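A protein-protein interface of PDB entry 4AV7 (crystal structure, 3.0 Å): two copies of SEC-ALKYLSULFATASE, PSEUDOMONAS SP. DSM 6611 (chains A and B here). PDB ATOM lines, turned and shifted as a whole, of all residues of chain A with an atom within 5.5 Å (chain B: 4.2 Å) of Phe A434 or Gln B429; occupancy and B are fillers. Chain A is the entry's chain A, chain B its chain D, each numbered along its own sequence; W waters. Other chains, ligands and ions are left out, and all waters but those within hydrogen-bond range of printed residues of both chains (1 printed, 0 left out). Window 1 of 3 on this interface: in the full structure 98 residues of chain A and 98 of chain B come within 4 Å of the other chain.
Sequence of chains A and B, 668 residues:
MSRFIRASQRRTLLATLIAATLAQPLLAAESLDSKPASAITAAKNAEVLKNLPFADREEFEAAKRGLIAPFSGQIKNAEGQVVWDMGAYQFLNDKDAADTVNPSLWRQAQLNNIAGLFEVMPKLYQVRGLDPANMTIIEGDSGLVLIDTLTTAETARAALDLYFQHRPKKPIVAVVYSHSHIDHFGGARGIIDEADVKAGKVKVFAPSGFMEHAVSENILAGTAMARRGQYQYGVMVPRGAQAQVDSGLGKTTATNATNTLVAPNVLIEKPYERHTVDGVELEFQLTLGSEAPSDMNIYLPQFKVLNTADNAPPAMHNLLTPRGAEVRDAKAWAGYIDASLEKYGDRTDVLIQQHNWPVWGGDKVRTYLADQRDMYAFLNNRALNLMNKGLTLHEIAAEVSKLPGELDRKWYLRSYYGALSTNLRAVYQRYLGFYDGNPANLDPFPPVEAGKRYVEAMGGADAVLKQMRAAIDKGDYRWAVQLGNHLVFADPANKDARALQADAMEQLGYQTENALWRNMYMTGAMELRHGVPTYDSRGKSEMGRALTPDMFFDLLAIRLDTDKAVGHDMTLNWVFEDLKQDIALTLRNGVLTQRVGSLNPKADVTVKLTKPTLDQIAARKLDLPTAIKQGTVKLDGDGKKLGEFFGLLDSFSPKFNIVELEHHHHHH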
ATOM      1  N   LEU A 320     -10.233 -19.144 -16.658  1.00  0.00           N
ATOM      2  CA  LEU A 320      -9.599 -19.111 -17.990  1.00  0.00           C
ATOM      3  C   LEU A 320      -9.245 -17.662 -18.380  1.00  0.00           C
ATOM      4  O   LEU A 320     -10.118 -16.892 -18.819  1.00  0.00           O
ATOM      5  CB  LEU A 320     -10.508 -19.723 -19.064  1.00  0.00           C
ATOM      6  CG  LEU A 320      -9.925 -19.706 -20.484  1.00  0.00           C
ATOM      7  CD1 LEU A 320      -9.080 -20.936 -20.824  1.00  0.00           C
ATOM      8  CD2 LEU A 320     -11.052 -19.600 -21.490  1.00  0.00           C
ATOM      9  N   ALA A 325      -3.923 -19.078 -21.131  1.00  0.00           N
ATOM     10  CA  ALA A 325      -3.148 -20.014 -20.306  1.00  0.00           C
ATOM     11  C   ALA A 325      -4.003 -21.257 -20.114  1.00  0.00           C
ATOM     12  O   ALA A 325      -5.139 -21.301 -20.589  1.00  0.00           O
ATOM     13  CB  ALA A 325      -2.778 -19.400 -18.967  1.00  0.00           C
ATOM     14  N   LEU A 393     -21.868 -24.776 -23.727  1.00  0.00           N
ATOM     15  CA  LEU A 393     -21.146 -23.737 -22.979  1.00  0.00           C
ATOM     16  C   LEU A 393     -21.831 -22.372 -22.983  1.00  0.00           C
ATOM     17  O   LEU A 393     -21.806 -21.652 -21.989  1.00  0.00           O
ATOM     18  CB  LEU A 393     -19.677 -23.624 -23.404  1.00  0.00           C
ATOM     19  CG  LEU A 393     -19.320 -23.212 -24.820  1.00  0.00           C
ATOM     20  CD1 LEU A 393     -17.859 -22.794 -24.857  1.00  0.00           C
ATOM     21  CD2 LEU A 393     -19.584 -24.359 -25.779  1.00  0.00           C
ATOM     22  N   TYR A 428     -16.950 -25.975 -18.723  1.00  0.00           N
ATOM     23  CA  TYR A 428     -17.227 -26.741 -19.924  1.00  0.00           C
ATOM     24  C   TYR A 428     -15.950 -27.094 -20.680  1.00  0.00           C
ATOM     25  O   TYR A 428     -15.739 -28.258 -21.073  1.00  0.00           O
ATOM     26  CB  TYR A 428     -18.163 -25.985 -20.863  1.00  0.00           C
ATOM     27  CG  TYR A 428     -18.786 -26.871 -21.925  1.00  0.00           C
ATOM     28  CD1 TYR A 428     -18.070 -27.236 -23.062  1.00  0.00           C
ATOM     29  CD2 TYR A 428     -20.076 -27.370 -21.771  1.00  0.00           C
ATOM     30  CE1 TYR A 428     -18.628 -28.055 -24.022  1.00  0.00           C
ATOM     31  CE2 TYR A 428     -20.645 -28.183 -22.729  1.00  0.00           C
ATOM     32  CZ  TYR A 428     -19.912 -28.519 -23.852  1.00  0.00           C
ATOM     33  OH  TYR A 428     -20.460 -29.324 -24.811  1.00  0.00           O
ATOM     34  N   GLN A 429     -15.101 -26.097 -20.888  1.00  0.00           N
ATOM     35  CA  GLN A 429     -13.862 -26.337 -21.596  1.00  0.00           C
ATOM     36  C   GLN A 429     -13.027 -27.403 -20.906  1.00  0.00           C
ATOM     37  O   GLN A 429     -12.500 -28.313 -21.570  1.00  0.00           O
ATOM     38  CB  GLN A 429     -13.048 -25.060 -21.753  1.00  0.00           C
ATOM     39  CG  GLN A 429     -11.757 -25.294 -22.528  1.00  0.00           C
ATOM     40  CD  GLN A 429     -10.864 -24.077 -22.558  1.00  0.00           C
ATOM     41  OE1 GLN A 429     -11.293 -22.992 -22.948  1.00  0.00           O
ATOM     42  NE2 GLN A 429      -9.610 -24.250 -22.164  1.00  0.00           N
ATOM     43  N   LEU A 432     -15.093 -30.914 -20.904  1.00  0.00           N
ATOM     44  CA  LEU A 432     -15.535 -31.382 -22.211  1.00  0.00           C
ATOM     45  C   LEU A 432     -14.765 -30.836 -23.403  1.00  0.00           C
ATOM     46  O   LEU A 432     -14.551 -31.554 -24.385  1.00  0.00           O
ATOM     47  CB  LEU A 432     -17.016 -31.092 -22.402  1.00  0.00           C
ATOM     48  CG  LEU A 432     -18.018 -31.795 -21.498  1.00  0.00           C
ATOM     49  CD1 LEU A 432     -19.405 -31.316 -21.835  1.00  0.00           C
ATOM     50  CD2 LEU A 432     -17.915 -33.309 -21.607  1.00  0.00           C
ATOM     51  N   GLY A 433     -14.378 -29.566 -23.344  1.00  0.00           N
ATOM     52  CA  GLY A 433     -13.611 -28.971 -24.434  1.00  0.00           C
ATOM     53  C   GLY A 433     -14.403 -27.959 -25.234  1.00  0.00           C
ATOM     54  O   GLY A 433     -15.578 -27.713 -24.927  1.00  0.00           O
ATOM     55  N   PHE A 434     -13.755 -27.383 -26.256  1.00  0.00           N
ATOM     56  CA  PHE A 434     -14.344 -26.339 -27.101  1.00  0.00           C
ATOM     57  C   PHE A 434     -15.493 -26.860 -27.972  1.00  0.00           C
ATOM     58  O   PHE A 434     -16.311 -26.078 -28.453  1.00  0.00           O
ATOM     59  CB  PHE A 434     -13.268 -25.667 -27.962  1.00  0.00           C
ATOM     60  CG  PHE A 434     -12.919 -26.430 -29.220  1.00  0.00           C
ATOM     61  CD1 PHE A 434     -11.954 -27.428 -29.206  1.00  0.00           C
ATOM     62  CD2 PHE A 434     -13.564 -26.144 -30.429  1.00  0.00           C
ATOM     63  CE1 PHE A 434     -11.646 -28.127 -30.363  1.00  0.00           C
ATOM     64  CE2 PHE A 434     -13.261 -26.844 -31.592  1.00  0.00           C
ATOM     65  CZ  PHE A 434     -12.299 -27.833 -31.557  1.00  0.00           C
ATOM     66  N   TYR A 435     -15.553 -28.175 -28.177  1.00  0.00           N
ATOM     67  CA  TYR A 435     -16.558 -28.765 -29.057  1.00  0.00           C
ATOM     68  C   TYR A 435     -17.827 -29.108 -28.296  1.00  0.00           C
ATOM     69  O   TYR A 435     -17.759 -29.873 -27.335  1.00  0.00           O
ATOM     70  CB  TYR A 435     -15.984 -30.012 -29.752  1.00  0.00           C
ATOM     71  CG  TYR A 435     -16.959 -30.765 -30.650  1.00  0.00           C
ATOM     72  CD1 TYR A 435     -17.585 -30.142 -31.748  1.00  0.00           C
ATOM     73  CD2 TYR A 435     -17.252 -32.109 -30.401  1.00  0.00           C
ATOM     74  CE1 TYR A 435     -18.486 -30.843 -32.553  1.00  0.00           C
ATOM     75  CE2 TYR A 435     -18.140 -32.813 -31.207  1.00  0.00           C
ATOM     76  CZ  TYR A 435     -18.755 -32.187 -32.282  1.00  0.00           C
ATOM     77  OH  TYR A 435     -19.629 -32.925 -33.058  1.00  0.00           O
ATOM     78  N   ASP A 436     -18.969 -28.571 -28.752  1.00  0.00           N
ATOM     79  CA  ASP A 436     -20.260 -28.707 -28.039  1.00  0.00           C
ATOM     80  C   ASP A 436     -21.029 -30.017 -28.256  1.00  0.00           C
ATOM     81  O   ASP A 436     -22.082 -30.244 -27.644  1.00  0.00           O
ATOM     82  CB  ASP A 436     -21.180 -27.496 -28.263  1.00  0.00           C
ATOM     83  CG  ASP A 436     -21.826 -27.480 -29.641  1.00  0.00           C
ATOM     84  OD1 ASP A 436     -21.272 -28.087 -30.583  1.00  0.00           O
ATOM     85  OD2 ASP A 436     -22.896 -26.841 -29.778  1.00  0.00           O
ATOM     86  N   ASN A 441     -20.780 -28.057 -35.686  1.00  0.00           N
ATOM     87  CA  ASN A 441     -19.790 -27.248 -35.051  1.00  0.00           C
ATOM     88  C   ASN A 441     -18.535 -28.062 -34.961  1.00  0.00           C
ATOM     89  O   ASN A 441     -17.601 -27.697 -34.258  1.00  0.00           O
ATOM     90  CB  ASN A 441     -20.267 -26.854 -33.659  1.00  0.00           C
ATOM     91  CG  ASN A 441     -21.465 -25.902 -33.691  1.00  0.00           C
ATOM     92  OD1 ASN A 441     -22.395 -26.006 -32.857  1.00  0.00           O
ATOM     93  ND2 ASN A 441     -21.444 -24.956 -34.655  1.00  0.00           N
ATOM     94  N   PRO A 444     -15.605 -25.635 -38.017  1.00  0.00           N
ATOM     95  CA  PRO A 444     -15.985 -24.253 -38.276  1.00  0.00           C
ATOM     96  C   PRO A 444     -14.991 -23.594 -39.199  1.00  0.00           C
ATOM     97  O   PRO A 444     -13.821 -24.000 -39.208  1.00  0.00           O
ATOM     98  CB  PRO A 444     -15.914 -23.606 -36.891  1.00  0.00           C
ATOM     99  CG  PRO A 444     -15.953 -24.739 -35.913  1.00  0.00           C
ATOM    100  CD  PRO A 444     -15.205 -25.831 -36.613  1.00  0.00           C
ATOM    101  N   LEU B 320      -8.146 -34.210 -28.131  1.00  0.00           N
ATOM    102  CA  LEU B 320      -9.409 -33.911 -27.460  1.00  0.00           C
ATOM    103  C   LEU B 320     -10.515 -34.825 -28.025  1.00  0.00           C
ATOM    104  O   LEU B 320     -10.955 -34.684 -29.171  1.00  0.00           O
ATOM    105  CB  LEU B 320      -9.752 -32.414 -27.590  1.00  0.00           C
ATOM    106  CG  LEU B 320     -11.067 -31.851 -27.026  1.00  0.00           C
ATOM    107  CD1 LEU B 320     -11.085 -31.675 -25.516  1.00  0.00           C
ATOM    108  CD2 LEU B 320     -11.366 -30.532 -27.722  1.00  0.00           C
ATOM    109  N   VAL B 327      -8.188 -31.968 -22.087  1.00  0.00           N
ATOM    110  CA  VAL B 327      -7.229 -32.012 -23.199  1.00  0.00           C
ATOM    111  C   VAL B 327      -5.980 -32.750 -22.822  1.00  0.00           C
ATOM    112  O   VAL B 327      -5.573 -32.762 -21.665  1.00  0.00           O
ATOM    113  CB  VAL B 327      -6.813 -30.666 -23.842  1.00  0.00           C
ATOM    114  CG1 VAL B 327      -7.690 -30.412 -25.034  1.00  0.00           C
ATOM    115  CG2 VAL B 327      -6.785 -29.486 -22.875  1.00  0.00           C
ATOM    116  N   LEU B 393      -7.607 -20.498 -33.409  1.00  0.00           N
ATOM    117  CA  LEU B 393      -7.808 -21.950 -33.575  1.00  0.00           C
ATOM    118  C   LEU B 393      -8.378 -22.442 -34.919  1.00  0.00           C
ATOM    119  O   LEU B 393      -7.994 -23.501 -35.395  1.00  0.00           O
ATOM    120  CB  LEU B 393      -8.631 -22.554 -32.408  1.00  0.00           C
ATOM    121  CG  LEU B 393     -10.093 -22.149 -32.165  1.00  0.00           C
ATOM    122  CD1 LEU B 393     -10.808 -23.175 -31.307  1.00  0.00           C
ATOM    123  CD2 LEU B 393     -10.178 -20.762 -31.547  1.00  0.00           C
ATOM    124  N   ARG B 425      -6.776 -27.439 -33.199  1.00  0.00           N
ATOM    125  CA  ARG B 425      -7.607 -26.634 -32.311  1.00  0.00           C
ATOM    126  C   ARG B 425      -7.388 -26.999 -30.825  1.00  0.00           C
ATOM    127  O   ARG B 425      -7.343 -26.114 -29.940  1.00  0.00           O
ATOM    128  CB  ARG B 425      -9.074 -26.769 -32.730  1.00  0.00           C
ATOM    129  CG  ARG B 425      -9.324 -26.181 -34.129  1.00  0.00           C
ATOM    130  CD  ARG B 425     -10.800 -26.059 -34.519  1.00  0.00           C
ATOM    131  NE  ARG B 425     -11.300 -27.190 -35.295  1.00  0.00           N
ATOM    132  CZ  ARG B 425     -11.648 -27.143 -36.578  1.00  0.00           C
ATOM    133  NH1 ARG B 425     -11.590 -26.013 -37.269  1.00  0.00           N
ATOM    134  NH2 ARG B 425     -12.085 -28.239 -37.169  1.00  0.00           N
ATOM    135  N   ALA B 426      -7.222 -28.299 -30.568  1.00  0.00           N
ATOM    136  CA  ALA B 426      -7.014 -28.804 -29.209  1.00  0.00           C
ATOM    137  C   ALA B 426      -5.717 -28.273 -28.559  1.00  0.00           C
ATOM    138  O   ALA B 426      -5.644 -28.107 -27.339  1.00  0.00           O
ATOM    139  CB  ALA B 426      -7.058 -30.325 -29.197  1.00  0.00           C
ATOM    140  N   VAL B 427      -4.695 -28.008 -29.364  1.00  0.00           N
ATOM    141  CA  VAL B 427      -3.484 -27.434 -28.828  1.00  0.00           C
ATOM    142  C   VAL B 427      -3.790 -25.979 -28.407  1.00  0.00           C
ATOM    143  O   VAL B 427      -3.381 -25.541 -27.327  1.00  0.00           O
ATOM    144  CB  VAL B 427      -2.313 -27.521 -29.843  1.00  0.00           C
ATOM    145  CG1 VAL B 427      -0.996 -27.045 -29.229  1.00  0.00           C
ATOM    146  CG2 VAL B 427      -2.152 -28.936 -30.370  1.00  0.00           C
ATOM    147  N   TYR B 428      -4.524 -25.250 -29.257  1.00  0.00           N
ATOM    148  CA  TYR B 428      -4.894 -23.874 -28.983  1.00  0.00           C
ATOM    149  C   TYR B 428      -5.741 -23.857 -27.716  1.00  0.00           C
ATOM    150  O   TYR B 428      -5.601 -22.968 -26.870  1.00  0.00           O
ATOM    151  CB  TYR B 428      -5.708 -23.307 -30.141  1.00  0.00           C
ATOM    152  CG  TYR B 428      -6.007 -21.806 -30.061  1.00  0.00           C
ATOM    153  CD1 TYR B 428      -6.975 -21.285 -29.201  1.00  0.00           C
ATOM    154  CD2 TYR B 428      -5.331 -20.920 -30.880  1.00  0.00           C
ATOM    155  CE1 TYR B 428      -7.224 -19.926 -29.163  1.00  0.00           C
ATOM    156  CE2 TYR B 428      -5.579 -19.569 -30.846  1.00  0.00           C
ATOM    157  CZ  TYR B 428      -6.512 -19.073 -29.997  1.00  0.00           C
ATOM    158  OH  TYR B 428      -6.699 -17.704 -30.014  1.00  0.00           O
ATOM    159  N   GLN B 429      -6.634 -24.838 -27.592  1.00  0.00           N
ATOM    160  CA  GLN B 429      -7.439 -24.968 -26.369  1.00  0.00           C
ATOM    161  C   GLN B 429      -6.534 -25.080 -25.154  1.00  0.00           C
ATOM    162  O   GLN B 429      -6.659 -24.270 -24.248  1.00  0.00           O
ATOM    163  CB  GLN B 429      -8.399 -26.154 -26.434  1.00  0.00           C
ATOM    164  CG  GLN B 429      -9.194 -26.318 -25.166  1.00  0.00           C
ATOM    165  CD  GLN B 429     -10.205 -27.441 -25.253  1.00  0.00           C
ATOM    166  OE1 GLN B 429     -11.011 -27.482 -26.191  1.00  0.00           O
ATOM    167  NE2 GLN B 429     -10.181 -28.368 -24.265  1.00  0.00           N
ATOM    168  N   ARG B 430      -5.615 -26.056 -25.173  1.00  0.00           N
ATOM    169  CA  ARG B 430      -4.742 -26.382 -24.040  1.00  0.00           C
ATOM    170  C   ARG B 430      -3.892 -25.194 -23.557  1.00  0.00           C
ATOM    171  O   ARG B 430      -3.825 -24.896 -22.347  1.00  0.00           O
ATOM    172  CB  ARG B 430      -3.816 -27.526 -24.411  1.00  0.00           C
ATOM    173  CG  ARG B 430      -3.260 -28.239 -23.188  1.00  0.00           C
ATOM    174  CD  ARG B 430      -2.216 -29.297 -23.497  1.00  0.00           C
ATOM    175  NE  ARG B 430      -0.889 -28.738 -23.327  1.00  0.00           N
ATOM    176  CZ  ARG B 430      -0.191 -28.833 -22.202  1.00  0.00           C
ATOM    177  NH1 ARG B 430      -0.722 -29.484 -21.156  1.00  0.00           N
ATOM    178  NH2 ARG B 430       1.034 -28.278 -22.131  1.00  0.00           N
ATOM    179  N   TYR B 431      -3.257 -24.507 -24.509  1.00  0.00           N
ATOM    180  CA  TYR B 431      -2.365 -23.416 -24.177  1.00  0.00           C
ATOM    181  C   TYR B 431      -3.073 -22.100 -23.946  1.00  0.00           C
ATOM    182  O   TYR B 431      -2.571 -21.303 -23.161  1.00  0.00           O
ATOM    183  CB  TYR B 431      -1.249 -23.255 -25.226  1.00  0.00           C
ATOM    184  CG  TYR B 431      -0.150 -24.336 -25.154  1.00  0.00           C
ATOM    185  CD1 TYR B 431       0.998 -24.171 -24.342  1.00  0.00           C
ATOM    186  CD2 TYR B 431      -0.265 -25.524 -25.895  1.00  0.00           C
ATOM    187  CE1 TYR B 431       1.982 -25.154 -24.273  1.00  0.00           C
ATOM    188  CE2 TYR B 431       0.715 -26.511 -25.827  1.00  0.00           C
ATOM    189  CZ  TYR B 431       1.834 -26.330 -25.020  1.00  0.00           C
ATOM    190  OH  TYR B 431       2.780 -27.335 -24.989  1.00  0.00           O
ATOM    191  N   LEU B 432      -4.215 -21.856 -24.607  1.00  0.00           N
ATOM    192  CA  LEU B 432      -4.830 -20.504 -24.624  1.00  0.00           C
ATOM    193  C   LEU B 432      -6.339 -20.476 -24.345  1.00  0.00           C
ATOM    194  O   LEU B 432      -6.895 -19.474 -23.860  1.00  0.00           O
ATOM    195  CB  LEU B 432      -4.564 -19.799 -25.964  1.00  0.00           C
ATOM    196  CG  LEU B 432      -3.179 -19.440 -26.482  1.00  0.00           C
ATOM    197  CD1 LEU B 432      -3.365 -18.827 -27.857  1.00  0.00           C
ATOM    198  CD2 LEU B 432      -2.499 -18.432 -25.586  1.00  0.00           C
ATOM    199  N   GLY B 433      -7.014 -21.557 -24.684  1.00  0.00           N
ATOM    200  CA  GLY B 433      -8.402 -21.665 -24.308  1.00  0.00           C
ATOM    201  C   GLY B 433      -9.317 -21.494 -25.483  1.00  0.00           C
ATOM    202  O   GLY B 433      -8.852 -21.285 -26.618  1.00  0.00           O
HETATM  203  O   HOH W   1      -7.044 -23.151 -21.832  1.00  0.00           O
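The backbone carbonyl oxygen (O) of Tyr B431 sits close to the backbone NH (N) of Ala A325 (3.3 Å). The backbone NH of Phe A434 is in hydrogen-bond range of the side-chain amide oxygen of Gln B429, 2.7 Å away.
O of Tyr A428 lies within hydrogen-bond range of N of Gly A433, 3.0 Å away. O of Tyr B428 is in hydrogen-bond range of N of Gly B433 (3.0 Å). The guanidinium group (NH2) of Arg B430 is in hydrogen-bond range of the side-chain hydroxyl (OH) of Tyr B431 (3.5 Å).
Among the printed residues, pairs that only touch across the chains: Leu A320 with Gly B433 (3.6 Å), Ala A325 with Leu B432 (3.9 Å), Gln A429 with Gln B429 (3.6 Å), Gln A429 with Gly B433 (3.5 Å), Leu A432 with Leu B320 (3.6 Å), Gly A433 with Leu B320 (3.9 Å), Gly A433 with Gln B429 (3.5 Å), Phe A434 with Leu B320 (3.5 Å), Phe A434 with Arg B425 (3.6 Å) and Pro A444 with Arg B425 (3.6 Å).
Tyr A428 touches none of the printed residues of chain B. Of chain B, only Leu B320, Arg B425 and Gln B429 come within 4 Å of Phe A434. Asp A436 touches none of the printed residues of chain B. Of the printed residues of chain A, Leu B320 touches Leu A432, Gly A433 and Phe A434. Of the printed residues of chain A, Arg B425 touches Phe A434 and Pro A444. Printed residues of chain A within 4 Å of Gln B429: Gln A429 (3.6 Å), Gly A433 (3.5 Å) and Phe A434 (2.7 Å). Of the printed residues of chain A, Leu B432 touches Ala A325. Of the printed residues of chain A, Gly B433 touches Leu A320 and Gln A429. The nearest residue of chain A that does not touch Gln B429 is Ala A325 (5.0 Å).
Hydrophobic or aromatic side chains of chain B that line the printed part of chain A: Leu B320. Of the 12 printed residues of chain A, 7 touch a printed residue of chain B. Hydrophobic or aromatic side chains of chain A that line the printed part of chain B: Leu A320, Phe A434 and Pro A444. Among the printed residues, no Asp or Glu carboxylate lies within 4 Å of a Lys or Arg side-chain nitrogen of the other chain.
Leu A320 touches Gly B433, and with the chains exchanged Gly A433 touches Leu B320. Gln B429 touches its own counterpart, Gln A429. Gln A429 touches Gly B433, and with the chains exchanged Gly A433 touches Gln B429. Leu A432 touches Leu B320, but with the chains exchanged Leu A320 does not touch Leu B432 (4.02 Å). Positions printed for both chains: 320, 393, 428, 429, 432 and 433.
Water W1 lies within hydrogen-bond range of the backbone carbonyl oxygen (O) of Gln B429, the side-chain amide nitrogen (NE2) of Gln A429, the backbone carbonyl oxygen (O) of Ala A325 and the backbone NH (N) of Gly B433.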
